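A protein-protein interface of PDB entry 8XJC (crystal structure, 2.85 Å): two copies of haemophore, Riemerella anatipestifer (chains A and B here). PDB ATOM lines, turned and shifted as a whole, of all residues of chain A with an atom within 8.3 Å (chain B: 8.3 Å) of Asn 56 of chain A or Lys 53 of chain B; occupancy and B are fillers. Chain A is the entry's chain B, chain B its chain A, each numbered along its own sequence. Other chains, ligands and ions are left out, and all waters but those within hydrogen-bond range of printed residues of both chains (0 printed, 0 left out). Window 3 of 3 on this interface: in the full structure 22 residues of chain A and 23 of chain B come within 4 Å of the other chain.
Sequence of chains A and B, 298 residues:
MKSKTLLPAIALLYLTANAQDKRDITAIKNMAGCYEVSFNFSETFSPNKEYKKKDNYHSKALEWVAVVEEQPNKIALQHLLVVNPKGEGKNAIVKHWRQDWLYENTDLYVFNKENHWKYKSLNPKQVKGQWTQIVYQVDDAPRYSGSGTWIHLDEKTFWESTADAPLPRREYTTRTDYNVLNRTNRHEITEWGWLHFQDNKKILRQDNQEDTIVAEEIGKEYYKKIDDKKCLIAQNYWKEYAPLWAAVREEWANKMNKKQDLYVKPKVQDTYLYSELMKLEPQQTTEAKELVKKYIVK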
ATOM      1  N   PHE A  39     -16.952  13.393 -13.659  1.00  0.00           N
ATOM      2  CA  PHE A  39     -17.121  12.012 -13.296  1.00  0.00           C
ATOM      3  C   PHE A  39     -18.530  11.815 -12.832  1.00  0.00           C
ATOM      4  O   PHE A  39     -18.969  12.502 -11.952  1.00  0.00           O
ATOM      5  CB  PHE A  39     -16.165  11.639 -12.183  1.00  0.00           C
ATOM      6  CG  PHE A  39     -14.718  11.704 -12.554  1.00  0.00           C
ATOM      7  CD1 PHE A  39     -14.095  10.619 -13.131  1.00  0.00           C
ATOM      8  CD2 PHE A  39     -13.974  12.830 -12.281  1.00  0.00           C
ATOM      9  CE1 PHE A  39     -12.760  10.667 -13.458  1.00  0.00           C
ATOM     10  CE2 PHE A  39     -12.640  12.885 -12.604  1.00  0.00           C
ATOM     11  CZ  PHE A  39     -12.031  11.802 -13.191  1.00  0.00           C
ATOM     12  N   ASN A  40     -19.236  10.857 -13.409  1.00  0.00           N
ATOM     13  CA  ASN A  40     -20.635  10.674 -13.109  1.00  0.00           C
ATOM     14  C   ASN A  40     -21.011   9.213 -13.068  1.00  0.00           C
ATOM     15  O   ASN A  40     -20.709   8.486 -13.982  1.00  0.00           O
ATOM     16  CB  ASN A  40     -21.466  11.377 -14.182  1.00  0.00           C
ATOM     17  CG  ASN A  40     -21.308  12.868 -14.180  1.00  0.00           C
ATOM     18  OD1 ASN A  40     -21.848  13.555 -13.326  1.00  0.00           O
ATOM     19  ND2 ASN A  40     -20.590  13.380 -15.159  1.00  0.00           N
ATOM     20  N   PHE A  41     -21.694   8.781 -12.017  1.00  0.00           N
ATOM     21  CA  PHE A  41     -22.119   7.392 -11.868  1.00  0.00           C
ATOM     22  C   PHE A  41     -23.497   7.277 -11.247  1.00  0.00           C
ATOM     23  O   PHE A  41     -23.782   7.967 -10.300  1.00  0.00           O
ATOM     24  CB  PHE A  41     -21.165   6.627 -10.965  1.00  0.00           C
ATOM     25  CG  PHE A  41     -19.799   6.418 -11.527  1.00  0.00           C
ATOM     26  CD1 PHE A  41     -19.546   5.359 -12.367  1.00  0.00           C
ATOM     27  CD2 PHE A  41     -18.760   7.251 -11.174  1.00  0.00           C
ATOM     28  CE1 PHE A  41     -18.285   5.152 -12.874  1.00  0.00           C
ATOM     29  CE2 PHE A  41     -17.496   7.053 -11.677  1.00  0.00           C
ATOM     30  CZ  PHE A  41     -17.256   5.997 -12.523  1.00  0.00           C
ATOM     31  N   SER A  42     -24.348   6.400 -11.769  1.00  0.00           N
ATOM     32  CA  SER A  42     -25.691   6.169 -11.221  1.00  0.00           C
ATOM     33  C   SER A  42     -26.031   4.738 -11.167  1.00  0.00           C
ATOM     34  O   SER A  42     -25.867   4.028 -12.129  1.00  0.00           O
ATOM     35  CB  SER A  42     -26.765   6.787 -12.064  1.00  0.00           C
ATOM     36  OG  SER A  42     -28.040   6.426 -11.579  1.00  0.00           O
ATOM     37  N   GLU A  43     -26.577   4.313 -10.056  1.00  0.00           N
ATOM     38  CA  GLU A  43     -26.939   2.937  -9.908  1.00  0.00           C
ATOM     39  C   GLU A  43     -28.226   2.622 -10.591  1.00  0.00           C
ATOM     40  O   GLU A  43     -29.141   3.426 -10.629  1.00  0.00           O
ATOM     41  CB  GLU A  43     -26.928   2.508  -8.454  1.00  0.00           C
ATOM     42  CG  GLU A  43     -25.547   2.217  -7.915  1.00  0.00           C
ATOM     43  CD  GLU A  43     -25.600   1.438  -6.630  1.00  0.00           C
ATOM     44  OE1 GLU A  43     -26.554   1.633  -5.861  1.00  0.00           O
ATOM     45  OE2 GLU A  43     -24.694   0.630  -6.388  1.00  0.00           O
ATOM     46  N   THR A  44     -28.299   1.430 -11.143  1.00  0.00           N
ATOM     47  CA  THR A  44     -29.444   1.056 -11.907  1.00  0.00           C
ATOM     48  C   THR A  44     -30.180  -0.155 -11.418  1.00  0.00           C
ATOM     49  O   THR A  44     -31.165  -0.028 -10.719  1.00  0.00           O
ATOM     50  CB  THR A  44     -28.989   0.786 -13.342  1.00  0.00           C
ATOM     51  OG1 THR A  44     -27.814  -0.026 -13.326  1.00  0.00           O
ATOM     52  CG2 THR A  44     -28.681   2.075 -14.062  1.00  0.00           C
ATOM     53  N   LYS A  53     -30.960   1.527  -3.840  1.00  0.00           N
ATOM     54  CA  LYS A  53     -29.953   2.196  -4.628  1.00  0.00           C
ATOM     55  C   LYS A  53     -29.246   3.263  -3.883  1.00  0.00           C
ATOM     56  O   LYS A  53     -29.854   4.034  -3.165  1.00  0.00           O
ATOM     57  CB  LYS A  53     -30.592   2.786  -5.880  1.00  0.00           C
ATOM     58  CG  LYS A  53     -30.872   1.776  -6.973  1.00  0.00           C
ATOM     59  CD  LYS A  53     -32.040   2.205  -7.842  1.00  0.00           C
ATOM     60  CE  LYS A  53     -31.816   3.570  -8.459  1.00  0.00           C
ATOM     61  NZ  LYS A  53     -32.919   3.937  -9.384  1.00  0.00           N
ATOM     62  N   LYS A  54     -27.952   3.343  -4.091  1.00  0.00           N
ATOM     63  CA  LYS A  54     -27.178   4.356  -3.437  1.00  0.00           C
ATOM     64  C   LYS A  54     -27.179   5.624  -4.240  1.00  0.00           C
ATOM     65  O   LYS A  54     -27.400   5.604  -5.438  1.00  0.00           O
ATOM     66  CB  LYS A  54     -25.787   3.839  -3.150  1.00  0.00           C
ATOM     67  CG  LYS A  54     -25.755   2.818  -2.028  1.00  0.00           C
ATOM     68  CD  LYS A  54     -24.342   2.366  -1.723  1.00  0.00           C
ATOM     69  CE  LYS A  54     -24.273   1.553  -0.440  1.00  0.00           C
ATOM     70  NZ  LYS A  54     -24.361   2.400   0.781  1.00  0.00           N
ATOM     71  N   ASP A  55     -26.956   6.743  -3.583  1.00  0.00           N
ATOM     72  CA  ASP A  55     -27.017   8.020  -4.250  1.00  0.00           C
ATOM     73  C   ASP A  55     -25.987   8.176  -5.336  1.00  0.00           C
ATOM     74  O   ASP A  55     -24.922   7.592  -5.272  1.00  0.00           O
ATOM     75  CB  ASP A  55     -26.897   9.146  -3.222  1.00  0.00           C
ATOM     76  CG  ASP A  55     -28.035   9.167  -2.243  1.00  0.00           C
ATOM     77  OD1 ASP A  55     -29.034   8.462  -2.469  1.00  0.00           O
ATOM     78  OD2 ASP A  55     -27.932   9.901  -1.245  1.00  0.00           O
ATOM     79  N   ASN A  56     -26.290   8.999  -6.323  1.00  0.00           N
ATOM     80  CA  ASN A  56     -25.393   9.149  -7.461  1.00  0.00           C
ATOM     81  C   ASN A  56     -24.120   9.922  -7.195  1.00  0.00           C
ATOM     82  O   ASN A  56     -24.081  10.760  -6.313  1.00  0.00           O
ATOM     83  CB  ASN A  56     -26.135   9.702  -8.684  1.00  0.00           C
ATOM     84  CG  ASN A  56     -27.286   8.836  -9.121  1.00  0.00           C
ATOM     85  OD1 ASN A  56     -28.085   9.252  -9.947  1.00  0.00           O
ATOM     86  ND2 ASN A  56     -27.376   7.630  -8.585  1.00  0.00           N
ATOM     87  N   TYR A  57     -23.082   9.653  -7.972  1.00  0.00           N
ATOM     88  CA  TYR A  57     -21.788  10.281  -7.778  1.00  0.00           C
ATOM     89  C   TYR A  57     -21.390  11.283  -8.813  1.00  0.00           C
ATOM     90  O   TYR A  57     -21.629  11.082  -9.981  1.00  0.00           O
ATOM     91  CB  TYR A  57     -20.735   9.193  -7.773  1.00  0.00           C
ATOM     92  CG  TYR A  57     -19.311   9.644  -7.549  1.00  0.00           C
ATOM     93  CD1 TYR A  57     -18.839   9.885  -6.275  1.00  0.00           C
ATOM     94  CD2 TYR A  57     -18.430   9.784  -8.606  1.00  0.00           C
ATOM     95  CE1 TYR A  57     -17.542  10.283  -6.059  1.00  0.00           C
ATOM     96  CE2 TYR A  57     -17.129  10.181  -8.397  1.00  0.00           C
ATOM     97  CZ  TYR A  57     -16.694  10.427  -7.119  1.00  0.00           C
ATOM     98  OH  TYR A  57     -15.401  10.823  -6.889  1.00  0.00           O
ATOM     99  N   HIS A  58     -20.780  12.370  -8.379  1.00  0.00           N
ATOM    100  CA  HIS A  58     -20.265  13.362  -9.293  1.00  0.00           C
ATOM    101  C   HIS A  58     -18.974  13.911  -8.751  1.00  0.00           C
ATOM    102  O   HIS A  58     -18.876  14.193  -7.572  1.00  0.00           O
ATOM    103  CB  HIS A  58     -21.256  14.477  -9.571  1.00  0.00           C
ATOM    104  CG  HIS A  58     -20.693  15.594 -10.389  1.00  0.00           C
ATOM    105  ND1 HIS A  58     -20.477  15.489 -11.744  1.00  0.00           N
ATOM    106  CD2 HIS A  58     -20.300  16.840 -10.042  1.00  0.00           C
ATOM    107  CE1 HIS A  58     -19.974  16.622 -12.197  1.00  0.00           C
ATOM    108  NE2 HIS A  58     -19.856  17.459 -11.184  1.00  0.00           N
ATOM    109  N   SER A  59     -17.971  14.019  -9.601  1.00  0.00           N
ATOM    110  CA  SER A  59     -16.712  14.605  -9.228  1.00  0.00           C
ATOM    111  C   SER A  59     -16.255  15.387 -10.419  1.00  0.00           C
ATOM    112  O   SER A  59     -16.892  15.378 -11.449  1.00  0.00           O
ATOM    113  CB  SER A  59     -15.689  13.560  -8.881  1.00  0.00           C
ATOM    114  OG  SER A  59     -14.460  14.144  -8.506  1.00  0.00           O
ATOM    115  N   ARG A 170     -14.371   5.313  -4.390  1.00  0.00           N
ATOM    116  CA  ARG A 170     -15.693   5.823  -4.151  1.00  0.00           C
ATOM    117  C   ARG A 170     -16.557   4.727  -3.630  1.00  0.00           C
ATOM    118  O   ARG A 170     -17.600   4.976  -3.056  1.00  0.00           O
ATOM    119  CB  ARG A 170     -16.254   6.384  -5.442  1.00  0.00           C
ATOM    120  CG  ARG A 170     -16.280   5.406  -6.587  1.00  0.00           C
ATOM    121  CD  ARG A 170     -16.890   6.004  -7.839  1.00  0.00           C
ATOM    122  NE  ARG A 170     -16.811   5.024  -8.908  1.00  0.00           N
ATOM    123  CZ  ARG A 170     -17.787   4.190  -9.228  1.00  0.00           C
ATOM    124  NH1 ARG A 170     -18.942   4.245  -8.592  1.00  0.00           N
ATOM    125  NH2 ARG A 170     -17.609   3.317 -10.198  1.00  0.00           N
ATOM    126  N   GLU A 171     -16.111   3.500  -3.790  1.00  0.00           N
ATOM    127  CA  GLU A 171     -16.912   2.369  -3.387  1.00  0.00           C
ATOM    128  C   GLU A 171     -16.397   1.663  -2.158  1.00  0.00           C
ATOM    129  O   GLU A 171     -17.166   1.304  -1.293  1.00  0.00           O
ATOM    130  CB  GLU A 171     -17.027   1.421  -4.560  1.00  0.00           C
ATOM    131  CG  GLU A 171     -17.775   2.006  -5.743  1.00  0.00           C
ATOM    132  CD  GLU A 171     -19.230   2.279  -5.433  1.00  0.00           C
ATOM    133  OE1 GLU A 171     -19.973   1.318  -5.183  1.00  0.00           O
ATOM    134  OE2 GLU A 171     -19.637   3.453  -5.456  1.00  0.00           O
ATOM    135  N   GLU A 217     -24.331  -0.387 -12.085  1.00  0.00           N
ATOM    136  CA  GLU A 217     -24.249   1.045 -12.203  1.00  0.00           C
ATOM    137  C   GLU A 217     -23.960   1.469 -13.599  1.00  0.00           C
ATOM    138  O   GLU A 217     -23.507   0.682 -14.406  1.00  0.00           O
ATOM    139  CB  GLU A 217     -23.143   1.584 -11.322  1.00  0.00           C
ATOM    140  CG  GLU A 217     -21.743   1.281 -11.805  1.00  0.00           C
ATOM    141  CD  GLU A 217     -20.685   1.901 -10.930  1.00  0.00           C
ATOM    142  OE1 GLU A 217     -21.040   2.619  -9.979  1.00  0.00           O
ATOM    143  OE2 GLU A 217     -19.497   1.666 -11.192  1.00  0.00           O
ATOM    144  N   ILE A 218     -24.240   2.721 -13.902  1.00  0.00           N
ATOM    145  CA  ILE A 218     -23.926   3.254 -15.203  1.00  0.00           C
ATOM    146  C   ILE A 218     -23.030   4.423 -14.940  1.00  0.00           C
ATOM    147  O   ILE A 218     -23.265   5.184 -14.036  1.00  0.00           O
ATOM    148  CB  ILE A 218     -25.177   3.680 -15.978  1.00  0.00           C
ATOM    149  CG1 ILE A 218     -25.881   2.460 -16.553  1.00  0.00           C
ATOM    150  CG2 ILE A 218     -24.839   4.614 -17.124  1.00  0.00           C
ATOM    151  CD1 ILE A 218     -25.155   1.847 -17.723  1.00  0.00           C
ATOM    152  N   SER B  42     -34.350   2.343 -15.723  1.00  0.00           N
ATOM    153  CA  SER B  42     -33.865   3.109 -14.571  1.00  0.00           C
ATOM    154  C   SER B  42     -33.382   4.460 -14.921  1.00  0.00           C
ATOM    155  O   SER B  42     -32.529   4.620 -15.763  1.00  0.00           O
ATOM    156  CB  SER B  42     -32.692   2.442 -13.879  1.00  0.00           C
ATOM    157  OG  SER B  42     -32.269   3.198 -12.767  1.00  0.00           O
ATOM    158  N   GLU B  43     -33.900   5.450 -14.235  1.00  0.00           N
ATOM    159  CA  GLU B  43     -33.454   6.787 -14.452  1.00  0.00           C
ATOM    160  C   GLU B  43     -32.118   6.974 -13.830  1.00  0.00           C
ATOM    161  O   GLU B  43     -31.847   6.446 -12.773  1.00  0.00           O
ATOM    162  CB  GLU B  43     -34.470   7.772 -13.934  1.00  0.00           C
ATOM    163  CG  GLU B  43     -35.751   7.772 -14.715  1.00  0.00           C
ATOM    164  CD  GLU B  43     -36.595   8.950 -14.355  1.00  0.00           C
ATOM    165  OE1 GLU B  43     -36.341   9.555 -13.301  1.00  0.00           O
ATOM    166  OE2 GLU B  43     -37.501   9.269 -15.126  1.00  0.00           O
ATOM    167  N   THR B  44     -31.267   7.739 -14.488  1.00  0.00           N
ATOM    168  CA  THR B  44     -29.903   7.897 -14.041  1.00  0.00           C
ATOM    169  C   THR B  44     -29.485   9.313 -13.709  1.00  0.00           C
ATOM    170  O   THR B  44     -29.441   9.688 -12.556  1.00  0.00           O
ATOM    171  CB  THR B  44     -28.972   7.332 -15.136  1.00  0.00           C
ATOM    172  OG1 THR B  44     -29.346   7.857 -16.409  1.00  0.00           O
ATOM    173  CG2 THR B  44     -29.053   5.829 -15.189  1.00  0.00           C
ATOM    174  N   PHE B  45     -29.187  10.111 -14.717  1.00  0.00           N
ATOM    175  CA  PHE B  45     -28.702  11.459 -14.496  1.00  0.00           C
ATOM    176  C   PHE B  45     -29.628  12.577 -14.935  1.00  0.00           C
ATOM    177  O   PHE B  45     -30.444  12.386 -15.805  1.00  0.00           O
ATOM    178  CB  PHE B  45     -27.417  11.650 -15.265  1.00  0.00           C
ATOM    179  CG  PHE B  45     -26.383  10.600 -15.025  1.00  0.00           C
ATOM    180  CD1 PHE B  45     -25.693  10.552 -13.834  1.00  0.00           C
ATOM    181  CD2 PHE B  45     -26.065   9.693 -16.016  1.00  0.00           C
ATOM    182  CE1 PHE B  45     -24.732   9.598 -13.622  1.00  0.00           C
ATOM    183  CE2 PHE B  45     -25.104   8.733 -15.809  1.00  0.00           C
ATOM    184  CZ  PHE B  45     -24.435   8.686 -14.610  1.00  0.00           C
ATOM    185  N   SER B  46     -29.480  13.760 -14.363  1.00  0.00           N
ATOM    186  CA  SER B  46     -30.265  14.911 -14.777  1.00  0.00           C
ATOM    187  C   SER B  46     -29.478  16.159 -14.552  1.00  0.00           C
ATOM    188  O   SER B  46     -28.734  16.240 -13.592  1.00  0.00           O
ATOM    189  CB  SER B  46     -31.532  15.003 -13.971  1.00  0.00           C
ATOM    190  OG  SER B  46     -32.217  16.209 -14.219  1.00  0.00           O
ATOM    191  N   ASN B  48     -30.726  18.957 -13.660  1.00  0.00           N
ATOM    192  CA  ASN B  48     -31.317  19.621 -12.531  1.00  0.00           C
ATOM    193  C   ASN B  48     -30.834  18.850 -11.348  1.00  0.00           C
ATOM    194  O   ASN B  48     -31.083  17.669 -11.233  1.00  0.00           O
ATOM    195  CB  ASN B  48     -32.840  19.583 -12.626  1.00  0.00           C
ATOM    196  CG  ASN B  48     -33.523  20.213 -11.436  1.00  0.00           C
ATOM    197  OD1 ASN B  48     -32.923  20.963 -10.674  1.00  0.00           O
ATOM    198  ND2 ASN B  48     -34.800  19.917 -11.281  1.00  0.00           N
ATOM    199  N   LYS B  49     -30.144  19.513 -10.448  1.00  0.00           N
ATOM    200  CA  LYS B  49     -29.580  18.850  -9.298  1.00  0.00           C
ATOM    201  C   LYS B  49     -30.649  18.478  -8.320  1.00  0.00           C
ATOM    202  O   LYS B  49     -30.514  17.524  -7.565  1.00  0.00           O
ATOM    203  CB  LYS B  49     -28.555  19.797  -8.680  1.00  0.00           C
ATOM    204  CG  LYS B  49     -28.341  19.706  -7.177  1.00  0.00           C
ATOM    205  CD  LYS B  49     -27.471  18.530  -6.775  1.00  0.00           C
ATOM    206  CE  LYS B  49     -27.484  18.366  -5.265  1.00  0.00           C
ATOM    207  NZ  LYS B  49     -28.876  18.299  -4.736  1.00  0.00           N
ATOM    208  N   GLU B  50     -31.749  19.194  -8.361  1.00  0.00           N
ATOM    209  CA  GLU B  50     -32.804  18.970  -7.406  1.00  0.00           C
ATOM    210  C   GLU B  50     -33.771  17.936  -7.891  1.00  0.00           C
ATOM    211  O   GLU B  50     -34.803  17.726  -7.276  1.00  0.00           O
ATOM    212  CB  GLU B  50     -33.514  20.288  -7.183  1.00  0.00           C
ATOM    213  CG  GLU B  50     -32.587  21.480  -7.032  1.00  0.00           C
ATOM    214  CD  GLU B  50     -31.849  21.490  -5.712  1.00  0.00           C
ATOM    215  OE1 GLU B  50     -32.364  20.920  -4.731  1.00  0.00           O
ATOM    216  OE2 GLU B  50     -30.745  22.070  -5.658  1.00  0.00           O
ATOM    217  N   TYR B  51     -33.438  17.265  -8.978  1.00  0.00           N
ATOM    218  CA  TYR B  51     -34.335  16.296  -9.558  1.00  0.00           C
ATOM    219  C   TYR B  51     -34.524  15.072  -8.726  1.00  0.00           C
ATOM    220  O   TYR B  51     -33.582  14.552  -8.157  1.00  0.00           O
ATOM    221  CB  TYR B  51     -33.837  15.897 -10.926  1.00  0.00           C
ATOM    222  CG  TYR B  51     -34.722  14.923 -11.662  1.00  0.00           C
ATOM    223  CD1 TYR B  51     -35.915  15.334 -12.225  1.00  0.00           C
ATOM    224  CD2 TYR B  51     -34.357  13.597 -11.804  1.00  0.00           C
ATOM    225  CE1 TYR B  51     -36.728  14.448 -12.897  1.00  0.00           C
ATOM    226  CE2 TYR B  51     -35.164  12.708 -12.473  1.00  0.00           C
ATOM    227  CZ  TYR B  51     -36.347  13.142 -13.015  1.00  0.00           C
ATOM    228  OH  TYR B  51     -37.153  12.259 -13.683  1.00  0.00           O
ATOM    229  N   LYS B  52     -35.758  14.587  -8.676  1.00  0.00           N
ATOM    230  CA  LYS B  52     -36.051  13.377  -7.946  1.00  0.00           C
ATOM    231  C   LYS B  52     -36.308  12.272  -8.906  1.00  0.00           C
ATOM    232  O   LYS B  52     -37.268  12.307  -9.653  1.00  0.00           O
ATOM    233  CB  LYS B  52     -37.256  13.550  -7.036  1.00  0.00           C
ATOM    234  CG  LYS B  52     -37.016  14.464  -5.853  1.00  0.00           C
ATOM    235  CD  LYS B  52     -38.143  14.335  -4.849  1.00  0.00           C
ATOM    236  CE  LYS B  52     -39.491  14.540  -5.510  1.00  0.00           C
ATOM    237  NZ  LYS B  52     -40.572  14.546  -4.490  1.00  0.00           N
ATOM    238  N   LYS B  53     -35.458  11.267  -8.868  1.00  0.00           N
ATOM    239  CA  LYS B  53     -35.575  10.165  -9.777  1.00  0.00           C
ATOM    240  C   LYS B  53     -36.800   9.361  -9.533  1.00  0.00           C
ATOM    241  O   LYS B  53     -37.177   9.126  -8.403  1.00  0.00           O
ATOM    242  CB  LYS B  53     -34.342   9.273  -9.668  1.00  0.00           C
ATOM    243  CG  LYS B  53     -33.107   9.829 -10.347  1.00  0.00           C
ATOM    244  CD  LYS B  53     -31.835   9.324  -9.687  1.00  0.00           C
ATOM    245  CE  LYS B  53     -31.795   7.810  -9.615  1.00  0.00           C
ATOM    246  NZ  LYS B  53     -30.534   7.324  -9.000  1.00  0.00           N
ATOM    247  N   LYS B  54     -37.407   8.889 -10.599  1.00  0.00           N
ATOM    248  CA  LYS B  54     -38.572   8.081 -10.469  1.00  0.00           C
ATOM    249  C   LYS B  54     -38.189   6.655 -10.238  1.00  0.00           C
ATOM    250  O   LYS B  54     -37.056   6.274 -10.460  1.00  0.00           O
ATOM    251  CB  LYS B  54     -39.411   8.200 -11.710  1.00  0.00           C
ATOM    252  CG  LYS B  54     -40.614   9.106 -11.582  1.00  0.00           C
ATOM    253  CD  LYS B  54     -40.305  10.502 -12.065  1.00  0.00           C
ATOM    254  CE  LYS B  54     -41.567  11.335 -12.110  1.00  0.00           C
ATOM    255  NZ  LYS B  54     -41.254  12.722 -12.530  1.00  0.00           N
ATOM    256  N   ASP B  55     -39.139   5.856  -9.788  1.00  0.00           N
ATOM    257  CA  ASP B  55     -38.894   4.462  -9.515  1.00  0.00           C
ATOM    258  C   ASP B  55     -38.672   3.645 -10.747  1.00  0.00           C
ATOM    259  O   ASP B  55     -39.171   3.965 -11.812  1.00  0.00           O
ATOM    260  CB  ASP B  55     -40.057   3.894  -8.731  1.00  0.00           C
ATOM    261  CG  ASP B  55     -40.173   4.483  -7.342  1.00  0.00           C
ATOM    262  OD1 ASP B  55     -39.164   4.997  -6.817  1.00  0.00           O
ATOM    263  OD2 ASP B  55     -41.277   4.419  -6.768  1.00  0.00           O
ATOM    264  N   ASN B  56     -37.945   2.557 -10.608  1.00  0.00           N
ATOM    265  CA  ASN B  56     -37.581   1.766 -11.761  1.00  0.00           C
ATOM    266  C   ASN B  56     -38.716   0.936 -12.255  1.00  0.00           C
ATOM    267  O   ASN B  56     -39.526   0.465 -11.478  1.00  0.00           O
ATOM    268  CB  ASN B  56     -36.377   0.888 -11.445  1.00  0.00           C
ATOM    269  CG  ASN B  56     -35.104   1.671 -11.244  1.00  0.00           C
ATOM    270  OD1 ASN B  56     -34.057   1.091 -10.978  1.00  0.00           O
ATOM    271  ND2 ASN B  56     -35.177   2.985 -11.379  1.00  0.00           N
ATOM    272  N   ARG B 175     -46.503  10.497 -16.832  1.00  0.00           N
ATOM    273  CA  ARG B 175     -45.847  11.798 -16.829  1.00  0.00           C
ATOM    274  C   ARG B 175     -46.179  12.757 -17.942  1.00  0.00           C
ATOM    275  O   ARG B 175     -46.469  12.335 -19.042  1.00  0.00           O
ATOM    276  CB  ARG B 175     -44.325  11.597 -16.856  1.00  0.00           C
ATOM    277  CG  ARG B 175     -43.737  10.702 -15.796  1.00  0.00           C
ATOM    278  CD  ARG B 175     -42.263  10.505 -16.052  1.00  0.00           C
ATOM    279  NE  ARG B 175     -41.548  11.768 -16.078  1.00  0.00           N
ATOM    280  CZ  ARG B 175     -40.233  11.861 -15.979  1.00  0.00           C
ATOM    281  NH1 ARG B 175     -39.518  10.768 -15.839  1.00  0.00           N
ATOM    282  NH2 ARG B 175     -39.638  13.040 -16.010  1.00  0.00           N
ATOM    283  N   VAL B 214     -34.700  16.631 -19.168  1.00  0.00           N
ATOM    284  CA  VAL B 214     -35.225  16.539 -17.836  1.00  0.00           C
ATOM    285  C   VAL B 214     -34.489  15.464 -17.107  1.00  0.00           C
ATOM    286  O   VAL B 214     -34.080  15.666 -15.983  1.00  0.00           O
ATOM    287  CB  VAL B 214     -36.716  16.213 -17.891  1.00  0.00           C
ATOM    288  CG1 VAL B 214     -37.294  16.050 -16.499  1.00  0.00           C
ATOM    289  CG2 VAL B 214     -37.459  17.284 -18.666  1.00  0.00           C
ATOM    290  N   ALA B 215     -34.302  14.328 -17.755  1.00  0.00           N
ATOM    291  CA  ALA B 215     -33.574  13.230 -17.150  1.00  0.00           C
ATOM    292  C   ALA B 215     -33.064  12.230 -18.138  1.00  0.00           C
ATOM    293  O   ALA B 215     -33.441  12.242 -19.281  1.00  0.00           O
ATOM    294  CB  ALA B 215     -34.418  12.538 -16.113  1.00  0.00           C
ATOM    295  N   GLU B 216     -32.174  11.367 -17.692  1.00  0.00           N
ATOM    296  CA  GLU B 216     -31.618  10.346 -18.548  1.00  0.00           C
ATOM    297  C   GLU B 216     -32.014   8.997 -18.006  1.00  0.00           C
ATOM    298  O   GLU B 216     -32.113   8.827 -16.816  1.00  0.00           O
ATOM    299  CB  GLU B 216     -30.105  10.458 -18.600  1.00  0.00           C
ATOM    300  CG  GLU B 216     -29.555  11.636 -19.356  1.00  0.00           C
ATOM    301  CD  GLU B 216     -28.065  11.516 -19.536  1.00  0.00           C
ATOM    302  OE1 GLU B 216     -27.547  10.406 -19.332  1.00  0.00           O
ATOM    303  OE2 GLU B 216     -27.416  12.523 -19.873  1.00  0.00           O
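The side-chain carboxylate (OE2) of Glu 43 of chain B is in salt-bridge range of the guanidinium group (NH1) of Arg 175 of chain B, at 2.6 Å. O of Phe 45 of chain B sits at hydrogen-bond distance from N of Glu 216 of chain B, 2.8 Å away. The side-chain amide oxygen of Asn 56 of chain A sits at hydrogen-bond distance from the side-chain hydroxyl of Ser 42 of chain A, 3.3 Å away.
Of the printed residues of chain B, Asn 56 of chain A touches Thr 44 and Lys 53. Of the printed residues of chain A, Lys 53 of chain B touches Ser 42 (3.7 Å) and Asn 56 (3.2 Å). Of the printed residues of chain B, Asn 40 of chain A touches Phe 45 (3.8 Å). Of the printed residues of chain A, Ser 42 of chain B touches Glu 43 (3.8 Å), Thr 44 (3.6 Å) and Lys 53 (3.5 Å). Asp 55 of chain B touches none of the printed residues of chain A. Lys 54 of chain A touches none of the printed residues of chain B. The nearest residue of chain B that does not touch Asn 56 of chain A is Phe 45 of chain B (4.7 Å).
Ser 42 of chain A touches Glu 43 of chain B, and with the chains exchanged Glu 43 of chain A touches Ser 42 of chain B. Ser 42 of chain A touches Thr 44 of chain B, and with the chains exchanged Thr 44 of chain A touches Ser 42 of chain B. Thr 44 of chain B touches its own counterpart, Thr 44 of chain A. Lys 53 of chain A touches Asn 56 of chain B, and with the chains exchanged Asn 56 of chain A touches Lys 53 of chain B. Positions printed for both chains: 42, 43, 44, 53, 54, 55 and 56.
The side-chain amide oxygen (OD1) of Asn 56 of chain A lies close to the backbone carbonyl oxygen (O) of Thr 44 of chain B (3.0 Å). The side-chain amino group of Lys 53 of chain B sits close to the side-chain amide nitrogen of Asn 56 of chain A, 3.2 Å away. OD1 of Asn 56 of chain B sits close to O of Thr 44 of chain A, 3.1 Å away. The side-chain amide nitrogen (ND2) of Asn 56 of chain B lies close to the side-chain amino group (NZ) of Lys 53 of chain A, 3.2 Å away.
Of the 17 printed residues of chain A, 8 touch a printed residue of chain B. Printed residues of chain B that touch a printed residue of chain A: Ser 42, Glu 43, Thr 44, Phe 45, Lys 53 and Asn 56. Among the printed residues, 15 pairs touch across the chains.
Among the printed residues, merely in contact across the chains: Ser 42 of chain A with Thr 44 of chain B (3.4 Å), Lys 53 of chain A with Ser 42 of chain B (3.5 Å), Phe 41 of chain A with Phe 45 of chain B (3.5 Å), Ser 42 of chain A with Phe 45 of chain B (3.6 Å), Thr 44 of chain A with Ser 42 of chain B (3.6 Å), Ser 42 of chain A with Lys 53 of chain B (3.7 Å), Ile 218 of chain A with Phe 45 of chain B (3.7 Å), Asn 40 of chain A with Phe 45 of chain B (3.8 Å), Glu 43 of chain A with Ser 42 of chain B (3.8 Å), Thr 44 of chain A with Thr 44 of chain B (3.9 Å) and Ser 42 of chain A with Glu 43 of chain B (3.99 Å).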
